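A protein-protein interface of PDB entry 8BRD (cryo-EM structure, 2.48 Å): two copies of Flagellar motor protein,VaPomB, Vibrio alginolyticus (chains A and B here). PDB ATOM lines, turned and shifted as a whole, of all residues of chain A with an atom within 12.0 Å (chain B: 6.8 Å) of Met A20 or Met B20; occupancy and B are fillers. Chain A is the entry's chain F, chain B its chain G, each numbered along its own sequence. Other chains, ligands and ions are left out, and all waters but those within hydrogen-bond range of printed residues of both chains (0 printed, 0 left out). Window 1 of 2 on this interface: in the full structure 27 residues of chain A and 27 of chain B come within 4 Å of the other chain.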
ATOM      1  N   THR A  11      -3.380   5.325  39.227  1.00  0.00           N
ATOM      2  CA  THR A  11      -3.747   4.398  38.160  1.00  0.00           C
ATOM      3  C   THR A  11      -3.974   5.135  36.846  1.00  0.00           C
ATOM      4  O   THR A  11      -3.543   4.678  35.781  1.00  0.00           O
ATOM      5  CB  THR A  11      -4.998   3.615  38.561  1.00  0.00           C
ATOM      6  OG1 THR A  11      -4.757   2.925  39.791  1.00  0.00           O
ATOM      7  CG2 THR A  11      -5.373   2.612  37.487  1.00  0.00           C
ATOM      8  N   PHE A  12      -4.644   6.285  36.908  1.00  0.00           N
ATOM      9  CA  PHE A  12      -4.949   7.058  35.714  1.00  0.00           C
ATOM     10  C   PHE A  12      -3.680   7.582  35.057  1.00  0.00           C
ATOM     11  O   PHE A  12      -3.561   7.562  33.830  1.00  0.00           O
ATOM     12  CB  PHE A  12      -5.898   8.202  36.074  1.00  0.00           C
ATOM     13  CG  PHE A  12      -6.353   9.016  34.897  1.00  0.00           C
ATOM     14  CD1 PHE A  12      -7.210   8.478  33.958  1.00  0.00           C
ATOM     15  CD2 PHE A  12      -5.934  10.323  34.740  1.00  0.00           C
ATOM     16  CE1 PHE A  12      -7.636   9.224  32.882  1.00  0.00           C
ATOM     17  CE2 PHE A  12      -6.354  11.070  33.664  1.00  0.00           C
ATOM     18  CZ  PHE A  12      -7.208  10.520  32.734  1.00  0.00           C
ATOM     19  N   ALA A  13      -2.716   8.046  35.854  1.00  0.00           N
ATOM     20  CA  ALA A  13      -1.463   8.522  35.276  1.00  0.00           C
ATOM     21  C   ALA A  13      -0.629   7.384  34.702  1.00  0.00           C
ATOM     22  O   ALA A  13       0.002   7.547  33.655  1.00  0.00           O
ATOM     23  CB  ALA A  13      -0.655   9.287  36.312  1.00  0.00           C
ATOM     24  N   ASP A  14      -0.595   6.228  35.376  1.00  0.00           N
ATOM     25  CA  ASP A  14       0.100   5.078  34.803  1.00  0.00           C
ATOM     26  C   ASP A  14      -0.521   4.660  33.481  1.00  0.00           C
ATOM     27  O   ASP A  14       0.195   4.386  32.510  1.00  0.00           O
ATOM     28  CB  ASP A  14       0.107   3.908  35.783  1.00  0.00           C
ATOM     29  CG  ASP A  14       0.630   4.290  37.145  1.00  0.00           C
ATOM     30  OD1 ASP A  14       1.031   5.457  37.321  1.00  0.00           O
ATOM     31  OD2 ASP A  14       0.641   3.424  38.045  1.00  0.00           O
ATOM     32  N   LEU A  15      -1.852   4.624  33.416  1.00  0.00           N
ATOM     33  CA  LEU A  15      -2.527   4.278  32.172  1.00  0.00           C
ATOM     34  C   LEU A  15      -2.260   5.317  31.089  1.00  0.00           C
ATOM     35  O   LEU A  15      -2.017   4.965  29.928  1.00  0.00           O
ATOM     36  CB  LEU A  15      -4.025   4.132  32.433  1.00  0.00           C
ATOM     37  CG  LEU A  15      -4.978   4.156  31.245  1.00  0.00           C
ATOM     38  CD1 LEU A  15      -4.908   2.848  30.499  1.00  0.00           C
ATOM     39  CD2 LEU A  15      -6.390   4.428  31.725  1.00  0.00           C
ATOM     40  N   MET A  16      -2.288   6.600  31.451  1.00  0.00           N
ATOM     41  CA  MET A  16      -2.032   7.665  30.488  1.00  0.00           C
ATOM     42  C   MET A  16      -0.613   7.597  29.942  1.00  0.00           C
ATOM     43  O   MET A  16      -0.402   7.759  28.737  1.00  0.00           O
ATOM     44  CB  MET A  16      -2.290   9.023  31.141  1.00  0.00           C
ATOM     45  CG  MET A  16      -3.720   9.553  31.074  1.00  0.00           C
ATOM     46  SD  MET A  16      -4.693   9.049  29.642  1.00  0.00           S
ATOM     47  CE  MET A  16      -5.626   7.684  30.317  1.00  0.00           C
ATOM     48  N   SER A  17       0.376   7.357  30.806  1.00  0.00           N
ATOM     49  CA  SER A  17       1.760   7.295  30.347  1.00  0.00           C
ATOM     50  C   SER A  17       2.011   6.041  29.519  1.00  0.00           C
ATOM     51  O   SER A  17       2.768   6.073  28.540  1.00  0.00           O
ATOM     52  CB  SER A  17       2.714   7.360  31.538  1.00  0.00           C
ATOM     53  OG  SER A  17       2.479   6.300  32.440  1.00  0.00           O
ATOM     54  N   LEU A  18       1.378   4.927  29.894  1.00  0.00           N
ATOM     55  CA  LEU A  18       1.447   3.712  29.093  1.00  0.00           C
ATOM     56  C   LEU A  18       0.874   3.934  27.697  1.00  0.00           C
ATOM     57  O   LEU A  18       1.482   3.547  26.689  1.00  0.00           O
ATOM     58  CB  LEU A  18       0.698   2.603  29.828  1.00  0.00           C
ATOM     59  CG  LEU A  18       0.580   1.190  29.280  1.00  0.00           C
ATOM     60  CD1 LEU A  18       0.676   0.208  30.425  1.00  0.00           C
ATOM     61  CD2 LEU A  18      -0.750   1.051  28.567  1.00  0.00           C
ATOM     62  N   LEU A  19      -0.297   4.567  27.618  1.00  0.00           N
ATOM     63  CA  LEU A  19      -0.899   4.848  26.323  1.00  0.00           C
ATOM     64  C   LEU A  19      -0.079   5.855  25.533  1.00  0.00           C
ATOM     65  O   LEU A  19      -0.018   5.768  24.307  1.00  0.00           O
ATOM     66  CB  LEU A  19      -2.331   5.342  26.511  1.00  0.00           C
ATOM     67  CG  LEU A  19      -3.372   4.304  26.925  1.00  0.00           C
ATOM     68  CD1 LEU A  19      -4.755   4.917  26.896  1.00  0.00           C
ATOM     69  CD2 LEU A  19      -3.306   3.087  26.024  1.00  0.00           C
ATOM     70  N   MET A  20       0.551   6.815  26.212  1.00  0.00           N
ATOM     71  CA  MET A  20       1.525   7.679  25.554  1.00  0.00           C
ATOM     72  C   MET A  20       2.643   6.878  24.910  1.00  0.00           C
ATOM     73  O   MET A  20       2.988   7.112  23.748  1.00  0.00           O
ATOM     74  CB  MET A  20       2.119   8.662  26.556  1.00  0.00           C
ATOM     75  CG  MET A  20       2.570   9.967  25.959  1.00  0.00           C
ATOM     76  SD  MET A  20       3.420  10.951  27.198  1.00  0.00           S
ATOM     77  CE  MET A  20       4.541  11.892  26.164  1.00  0.00           C
ATOM     78  N   CYS A  21       3.230   5.939  25.653  1.00  0.00           N
ATOM     79  CA  CYS A  21       4.311   5.127  25.104  1.00  0.00           C
ATOM     80  C   CYS A  21       3.843   4.369  23.870  1.00  0.00           C
ATOM     81  O   CYS A  21       4.520   4.351  22.833  1.00  0.00           O
ATOM     82  CB  CYS A  21       4.827   4.156  26.166  1.00  0.00           C
ATOM     83  SG  CYS A  21       5.651   4.937  27.569  1.00  0.00           S
ATOM     84  N   PHE A  22       2.657   3.773  23.949  1.00  0.00           N
ATOM     85  CA  PHE A  22       2.184   2.961  22.836  1.00  0.00           C
ATOM     86  C   PHE A  22       1.708   3.790  21.649  1.00  0.00           C
ATOM     87  O   PHE A  22       1.814   3.332  20.510  1.00  0.00           O
ATOM     88  CB  PHE A  22       1.097   2.010  23.329  1.00  0.00           C
ATOM     89  CG  PHE A  22       1.654   0.814  24.038  1.00  0.00           C
ATOM     90  CD1 PHE A  22       2.064   0.914  25.357  1.00  0.00           C
ATOM     91  CD2 PHE A  22       1.832  -0.384  23.380  1.00  0.00           C
ATOM     92  CE1 PHE A  22       2.603  -0.165  26.013  1.00  0.00           C
ATOM     93  CE2 PHE A  22       2.371  -1.466  24.037  1.00  0.00           C
ATOM     94  CZ  PHE A  22       2.758  -1.355  25.349  1.00  0.00           C
ATOM     95  N   PHE A  23       1.237   5.016  21.870  1.00  0.00           N
ATOM     96  CA  PHE A  23       0.884   5.881  20.751  1.00  0.00           C
ATOM     97  C   PHE A  23       2.118   6.490  20.101  1.00  0.00           C
ATOM     98  O   PHE A  23       2.124   6.713  18.887  1.00  0.00           O
ATOM     99  CB  PHE A  23      -0.085   6.971  21.212  1.00  0.00           C
ATOM    100  CG  PHE A  23      -1.493   6.483  21.379  1.00  0.00           C
ATOM    101  CD1 PHE A  23      -2.100   5.737  20.386  1.00  0.00           C
ATOM    102  CD2 PHE A  23      -2.204   6.748  22.535  1.00  0.00           C
ATOM    103  CE1 PHE A  23      -3.386   5.273  20.539  1.00  0.00           C
ATOM    104  CE2 PHE A  23      -3.490   6.282  22.695  1.00  0.00           C
ATOM    105  CZ  PHE A  23      -4.082   5.546  21.693  1.00  0.00           C
ATOM    106  N   VAL A  24       3.175   6.742  20.878  1.00  0.00           N
ATOM    107  CA  VAL A  24       4.467   7.080  20.286  1.00  0.00           C
ATOM    108  C   VAL A  24       4.960   5.928  19.424  1.00  0.00           C
ATOM    109  O   VAL A  24       5.499   6.135  18.328  1.00  0.00           O
ATOM    110  CB  VAL A  24       5.489   7.442  21.380  1.00  0.00           C
ATOM    111  CG1 VAL A  24       6.868   7.648  20.777  1.00  0.00           C
ATOM    112  CG2 VAL A  24       5.060   8.689  22.112  1.00  0.00           C
ATOM    113  N   LEU A  25       4.785   4.696  19.905  1.00  0.00           N
ATOM    114  CA  LEU A  25       5.125   3.529  19.096  1.00  0.00           C
ATOM    115  C   LEU A  25       4.324   3.501  17.801  1.00  0.00           C
ATOM    116  O   LEU A  25       4.885   3.307  16.717  1.00  0.00           O
ATOM    117  CB  LEU A  25       4.874   2.252  19.888  1.00  0.00           C
ATOM    118  CG  LEU A  25       5.013   0.973  19.064  1.00  0.00           C
ATOM    119  CD1 LEU A  25       6.474   0.635  18.879  1.00  0.00           C
ATOM    120  CD2 LEU A  25       4.259  -0.177  19.694  1.00  0.00           C
ATOM    121  N   LEU A  26       3.007   3.686  17.897  1.00  0.00           N
ATOM    122  CA  LEU A  26       2.164   3.635  16.708  1.00  0.00           C
ATOM    123  C   LEU A  26       2.530   4.728  15.717  1.00  0.00           C
ATOM    124  O   LEU A  26       2.482   4.506  14.502  1.00  0.00           O
ATOM    125  CB  LEU A  26       0.694   3.741  17.101  1.00  0.00           C
ATOM    126  CG  LEU A  26       0.072   2.498  17.733  1.00  0.00           C
ATOM    127  CD1 LEU A  26      -1.205   2.860  18.463  1.00  0.00           C
ATOM    128  CD2 LEU A  26      -0.194   1.436  16.688  1.00  0.00           C
ATOM    129  N   LEU A  27       2.893   5.910  16.208  1.00  0.00           N
ATOM    130  CA  LEU A  27       3.360   6.982  15.343  1.00  0.00           C
ATOM    131  C   LEU A  27       4.781   6.760  14.844  1.00  0.00           C
ATOM    132  O   LEU A  27       5.210   7.457  13.918  1.00  0.00           O
ATOM    133  CB  LEU A  27       3.271   8.314  16.085  1.00  0.00           C
ATOM    134  CG  LEU A  27       3.191   9.584  15.245  1.00  0.00           C
ATOM    135  CD1 LEU A  27       1.836   9.699  14.582  1.00  0.00           C
ATOM    136  CD2 LEU A  27       3.455  10.781  16.124  1.00  0.00           C
ATOM    137  N   SER A  28       5.516   5.816  15.433  1.00  0.00           N
ATOM    138  CA  SER A  28       6.862   5.525  14.953  1.00  0.00           C
ATOM    139  C   SER A  28       6.833   4.854  13.584  1.00  0.00           C
ATOM    140  O   SER A  28       7.597   5.231  12.690  1.00  0.00           O
ATOM    141  CB  SER A  28       7.605   4.661  15.969  1.00  0.00           C
ATOM    142  OG  SER A  28       7.690   5.311  17.224  1.00  0.00           O
ATOM    143  N   PHE A  29       5.971   3.854  13.397  1.00  0.00           N
ATOM    144  CA  PHE A  29       5.801   3.232  12.086  1.00  0.00           C
ATOM    145  C   PHE A  29       4.637   3.835  11.314  1.00  0.00           C
ATOM    146  O   PHE A  29       3.799   3.113  10.770  1.00  0.00           O
ATOM    147  CB  PHE A  29       5.625   1.721  12.213  1.00  0.00           C
ATOM    148  CG  PHE A  29       4.689   1.293  13.308  1.00  0.00           C
ATOM    149  CD1 PHE A  29       3.335   1.185  13.070  1.00  0.00           C
ATOM    150  CD2 PHE A  29       5.165   0.949  14.556  1.00  0.00           C
ATOM    151  CE1 PHE A  29       2.474   0.774  14.059  1.00  0.00           C
ATOM    152  CE2 PHE A  29       4.305   0.537  15.547  1.00  0.00           C
ATOM    153  CZ  PHE A  29       2.959   0.450  15.294  1.00  0.00           C
ATOM    154  N   MET A  32       3.049  10.776   8.845  1.00  0.00           N
ATOM    155  CA  MET A  32       2.142  11.907   8.978  1.00  0.00           C
ATOM    156  C   MET A  32       1.987  12.620   7.642  1.00  0.00           C
ATOM    157  O   MET A  32       2.967  12.887   6.944  1.00  0.00           O
ATOM    158  CB  MET A  32       2.655  12.891  10.029  1.00  0.00           C
ATOM    159  CG  MET A  32       2.784  12.324  11.427  1.00  0.00           C
ATOM    160  SD  MET A  32       2.794  13.637  12.660  1.00  0.00           S
ATOM    161  CE  MET A  32       4.268  13.224  13.584  1.00  0.00           C
ATOM    162  N   MET A  44      -3.055  25.724  15.564  1.00  0.00           N
ATOM    163  CA  MET A  44      -2.409  25.902  16.861  1.00  0.00           C
ATOM    164  C   MET A  44      -1.718  27.254  16.951  1.00  0.00           C
ATOM    165  O   MET A  44      -1.706  27.880  18.015  1.00  0.00           O
ATOM    166  CB  MET A  44      -1.413  24.774  17.133  1.00  0.00           C
ATOM    167  CG  MET A  44      -1.971  23.385  16.972  1.00  0.00           C
ATOM    168  SD  MET A  44      -2.833  22.798  18.433  1.00  0.00           S
ATOM    169  CE  MET A  44      -2.468  21.047  18.340  1.00  0.00           C
ATOM    170  N   LEU B  15      -0.882  16.123  32.269  1.00  0.00           N
ATOM    171  CA  LEU B  15       0.133  16.254  31.230  1.00  0.00           C
ATOM    172  C   LEU B  15       0.204  15.004  30.370  1.00  0.00           C
ATOM    173  O   LEU B  15       0.345  15.081  29.145  1.00  0.00           O
ATOM    174  CB  LEU B  15       1.489  16.538  31.879  1.00  0.00           C
ATOM    175  CG  LEU B  15       2.696  16.727  30.962  1.00  0.00           C
ATOM    176  CD1 LEU B  15       2.481  17.906  30.052  1.00  0.00           C
ATOM    177  CD2 LEU B  15       3.954  16.900  31.785  1.00  0.00           C
ATOM    178  N   MET B  16       0.123  13.833  31.006  1.00  0.00           N
ATOM    179  CA  MET B  16       0.123  12.580  30.265  1.00  0.00           C
ATOM    180  C   MET B  16      -1.090  12.468  29.353  1.00  0.00           C
ATOM    181  O   MET B  16      -0.958  12.018  28.212  1.00  0.00           O
ATOM    182  CB  MET B  16       0.176  11.403  31.237  1.00  0.00           C
ATOM    183  CG  MET B  16       1.554  11.013  31.786  1.00  0.00           C
ATOM    184  SD  MET B  16       2.987  11.159  30.692  1.00  0.00           S
ATOM    185  CE  MET B  16       3.497  12.858  30.928  1.00  0.00           C
ATOM    186  N   SER B  17      -2.267  12.879  29.831  1.00  0.00           N
ATOM    187  CA  SER B  17      -3.460  12.903  28.990  1.00  0.00           C
ATOM    188  C   SER B  17      -3.274  13.840  27.805  1.00  0.00           C
ATOM    189  O   SER B  17      -3.623  13.507  26.668  1.00  0.00           O
ATOM    190  CB  SER B  17      -4.672  13.331  29.816  1.00  0.00           C
ATOM    191  OG  SER B  17      -4.699  12.681  31.069  1.00  0.00           O
ATOM    192  N   LEU B  18      -2.724  15.028  28.063  1.00  0.00           N
ATOM    193  CA  LEU B  18      -2.510  16.006  27.002  1.00  0.00           C
ATOM    194  C   LEU B  18      -1.576  15.462  25.929  1.00  0.00           C
ATOM    195  O   LEU B  18      -1.867  15.554  24.733  1.00  0.00           O
ATOM    196  CB  LEU B  18      -1.953  17.299  27.598  1.00  0.00           C
ATOM    197  CG  LEU B  18      -2.954  18.198  28.326  1.00  0.00           C
ATOM    198  CD1 LEU B  18      -2.245  19.255  29.146  1.00  0.00           C
ATOM    199  CD2 LEU B  18      -3.868  18.851  27.312  1.00  0.00           C
ATOM    200  N   LEU B  19      -0.453  14.877  26.343  1.00  0.00           N
ATOM    201  CA  LEU B  19       0.510  14.353  25.377  1.00  0.00           C
ATOM    202  C   LEU B  19      -0.047  13.144  24.638  1.00  0.00           C
ATOM    203  O   LEU B  19       0.136  13.005  23.424  1.00  0.00           O
ATOM    204  CB  LEU B  19       1.815  14.009  26.088  1.00  0.00           C
ATOM    205  CG  LEU B  19       2.567  15.208  26.667  1.00  0.00           C
ATOM    206  CD1 LEU B  19       3.403  14.801  27.860  1.00  0.00           C
ATOM    207  CD2 LEU B  19       3.430  15.852  25.604  1.00  0.00           C
ATOM    208  N   MET B  20      -0.750  12.267  25.353  1.00  0.00           N
ATOM    209  CA  MET B  20      -1.394  11.117  24.730  1.00  0.00           C
ATOM    210  C   MET B  20      -2.383  11.546  23.656  1.00  0.00           C
ATOM    211  O   MET B  20      -2.401  10.996  22.550  1.00  0.00           O
ATOM    212  CB  MET B  20      -2.099  10.301  25.806  1.00  0.00           C
ATOM    213  CG  MET B  20      -2.398   8.887  25.427  1.00  0.00           C
ATOM    214  SD  MET B  20      -3.838   8.369  26.359  1.00  0.00           S
ATOM    215  CE  MET B  20      -5.023   9.575  25.788  1.00  0.00           C
ATOM    216  N   CYS B  21      -3.221  12.534  23.964  1.00  0.00           N
ATOM    217  CA  CYS B  21      -4.218  12.964  22.994  1.00  0.00           C
ATOM    218  C   CYS B  21      -3.588  13.773  21.870  1.00  0.00           C
ATOM    219  O   CYS B  21      -4.109  13.783  20.751  1.00  0.00           O
ATOM    220  CB  CYS B  21      -5.319  13.748  23.696  1.00  0.00           C
ATOM    221  SG  CYS B  21      -6.531  12.684  24.499  1.00  0.00           S
ATOM    222  N   PHE B  22      -2.455  14.426  22.129  1.00  0.00           N
ATOM    223  CA  PHE B  22      -1.692  15.024  21.039  1.00  0.00           C
ATOM    224  C   PHE B  22      -1.169  13.956  20.088  1.00  0.00           C
ATOM    225  O   PHE B  22      -1.160  14.146  18.867  1.00  0.00           O
ATOM    226  CB  PHE B  22      -0.541  15.860  21.596  1.00  0.00           C
ATOM    227  CG  PHE B  22       0.212  16.622  20.545  1.00  0.00           C
ATOM    228  CD1 PHE B  22      -0.439  17.539  19.740  1.00  0.00           C
ATOM    229  CD2 PHE B  22       1.564  16.416  20.354  1.00  0.00           C
ATOM    230  CE1 PHE B  22       0.244  18.236  18.773  1.00  0.00           C
ATOM    231  CE2 PHE B  22       2.252  17.112  19.385  1.00  0.00           C
ATOM    232  CZ  PHE B  22       1.592  18.022  18.595  1.00  0.00           C
ATOM    233  N   PHE B  23      -0.728  12.822  20.631  1.00  0.00           N
ATOM    234  CA  PHE B  23      -0.276  11.733  19.771  1.00  0.00           C
ATOM    235  C   PHE B  23      -1.441  11.097  19.027  1.00  0.00           C
ATOM    236  O   PHE B  23      -1.283  10.648  17.890  1.00  0.00           O
ATOM    237  CB  PHE B  23       0.485  10.692  20.589  1.00  0.00           C
ATOM    238  CG  PHE B  23       1.777  11.202  21.135  1.00  0.00           C
ATOM    239  CD1 PHE B  23       2.661  11.881  20.321  1.00  0.00           C
ATOM    240  CD2 PHE B  23       2.103  11.018  22.464  1.00  0.00           C
ATOM    241  CE1 PHE B  23       3.844  12.367  20.822  1.00  0.00           C
ATOM    242  CE2 PHE B  23       3.283  11.509  22.970  1.00  0.00           C
ATOM    243  CZ  PHE B  23       4.155  12.181  22.148  1.00  0.00           C
ATOM    244  N   VAL B  24      -2.621  11.051  19.648  1.00  0.00           N
ATOM    245  CA  VAL B  24      -3.815  10.603  18.930  1.00  0.00           C
ATOM    246  C   VAL B  24      -4.138  11.552  17.781  1.00  0.00           C
ATOM    247  O   VAL B  24      -4.492  11.114  16.677  1.00  0.00           O
ATOM    248  CB  VAL B  24      -5.009  10.454  19.893  1.00  0.00           C
ATOM    249  CG1 VAL B  24      -6.238   9.978  19.140  1.00  0.00           C
ATOM    250  CG2 VAL B  24      -4.673   9.477  20.994  1.00  0.00           C
ATOM    251  N   LEU B  25      -4.009  12.859  18.014  1.00  0.00           N
ATOM    252  CA  LEU B  25      -4.193  13.835  16.947  1.00  0.00           C
ATOM    253  C   LEU B  25      -3.196  13.611  15.817  1.00  0.00           C
ATOM    254  O   LEU B  25      -3.558  13.664  14.638  1.00  0.00           O
ATOM    255  CB  LEU B  25      -4.057  15.251  17.503  1.00  0.00           C
ATOM    256  CG  LEU B  25      -4.059  16.383  16.473  1.00  0.00           C
ATOM    257  CD1 LEU B  25      -5.412  16.518  15.815  1.00  0.00           C
ATOM    258  CD2 LEU B  25      -3.640  17.689  17.113  1.00  0.00           C
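Printed residues of chain B within 4 Å of Ser A17: Met B16. Printed residues of chain B within 4 Å of Leu A19: Met B20 (3.4 Å). Met A20 touches just these residues of chain B: Met B16 (3.5 Å), Leu B19 (3.5 Å), Met B20 (3.7 Å) and Phe B23 (3.4 Å). Cys A21 touches none of the printed residues of chain B. Leu A27 touches none of the printed residues of chain B. Met B16 touches three residues of chain A. Ser B17 touches just these residues of chain A: Phe A12 and Met A16. Leu B19 touches one residue of chain A. Val B24 touches one residue of chain A. Of the printed residues of chain A, Leu B25 touches Met A44 (3.8 Å). The nearest residue of chain B that does not touch Met A20 is Leu B15 (5.5 Å).
SD of Met A16 lies close to SD of Met B20, at 3.5 Å. SD of Met A20 sits close to SD of Met B16.
Among the printed residues, merely in contact across the chains: Met A16 with Ser B17 (3.3 Å), Leu A19 with Met B20 (3.4 Å), Met A16 with Met B16 (3.4 Å), Met A20 with Phe B23 (3.4 Å), Val A24 with Phe B23 (3.4 Å), Met A20 with Leu B19 (3.5 Å), Phe A12 with Ser B17 (3.5 Å), Phe A23 with Met B20 (3.6 Å), Met A20 with Met B20 (3.7 Å), Met A44 with Leu B25 (3.8 Å), Phe A23 with Val B24 (3.8 Å), Phe A23 with Phe B23 (3.8 Å), Ser A17 with Met B16 (3.8 Å) and Met A44 with Phe B22 (3.9 Å).
Met A16 touches Met B20, and with the chains exchanged Met A20 touches Met B16. Met B20 touches its own counterpart, Met A20. Met A20 touches Phe B23, and with the chains exchanged Phe A23 touches Met B20. Phe A23 touches Val B24, and with the chains exchanged Val A24 touches Phe B23. Of the 16 pairs that touch across the chains among the printed residues, 13 have their exchanged pair printed and touching as well.
Hydrophobic or aromatic side chains of chain B that line the printed part of chain A: Met B16, Leu B19, Met B20, Phe B22, Phe B23, Val B24 and Leu B25. Of the 21 printed residues of chain A, 8 touch a printed residue of chain B. Among the printed residues, 16 pairs touch across the chains.
The side-chain hydroxyl (OG) of Ser A17 lies within hydrogen-bond range of the backbone carbonyl oxygen (O) of Asp A14, at 3.0 Å. SG of Cys B21 sits close to O of Ser B17 (3.7 Å). O of Ala A13 lies within hydrogen-bond range of OG of Ser A17 (3.0 Å). OG of Ser A28 lies within hydrogen-bond range of O of Val A24, at 2.6 Å. The side-chain sulfur of Cys A21 lies within hydrogen-bond range of the backbone carbonyl oxygen of Ser A17, 3.2 Å away.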
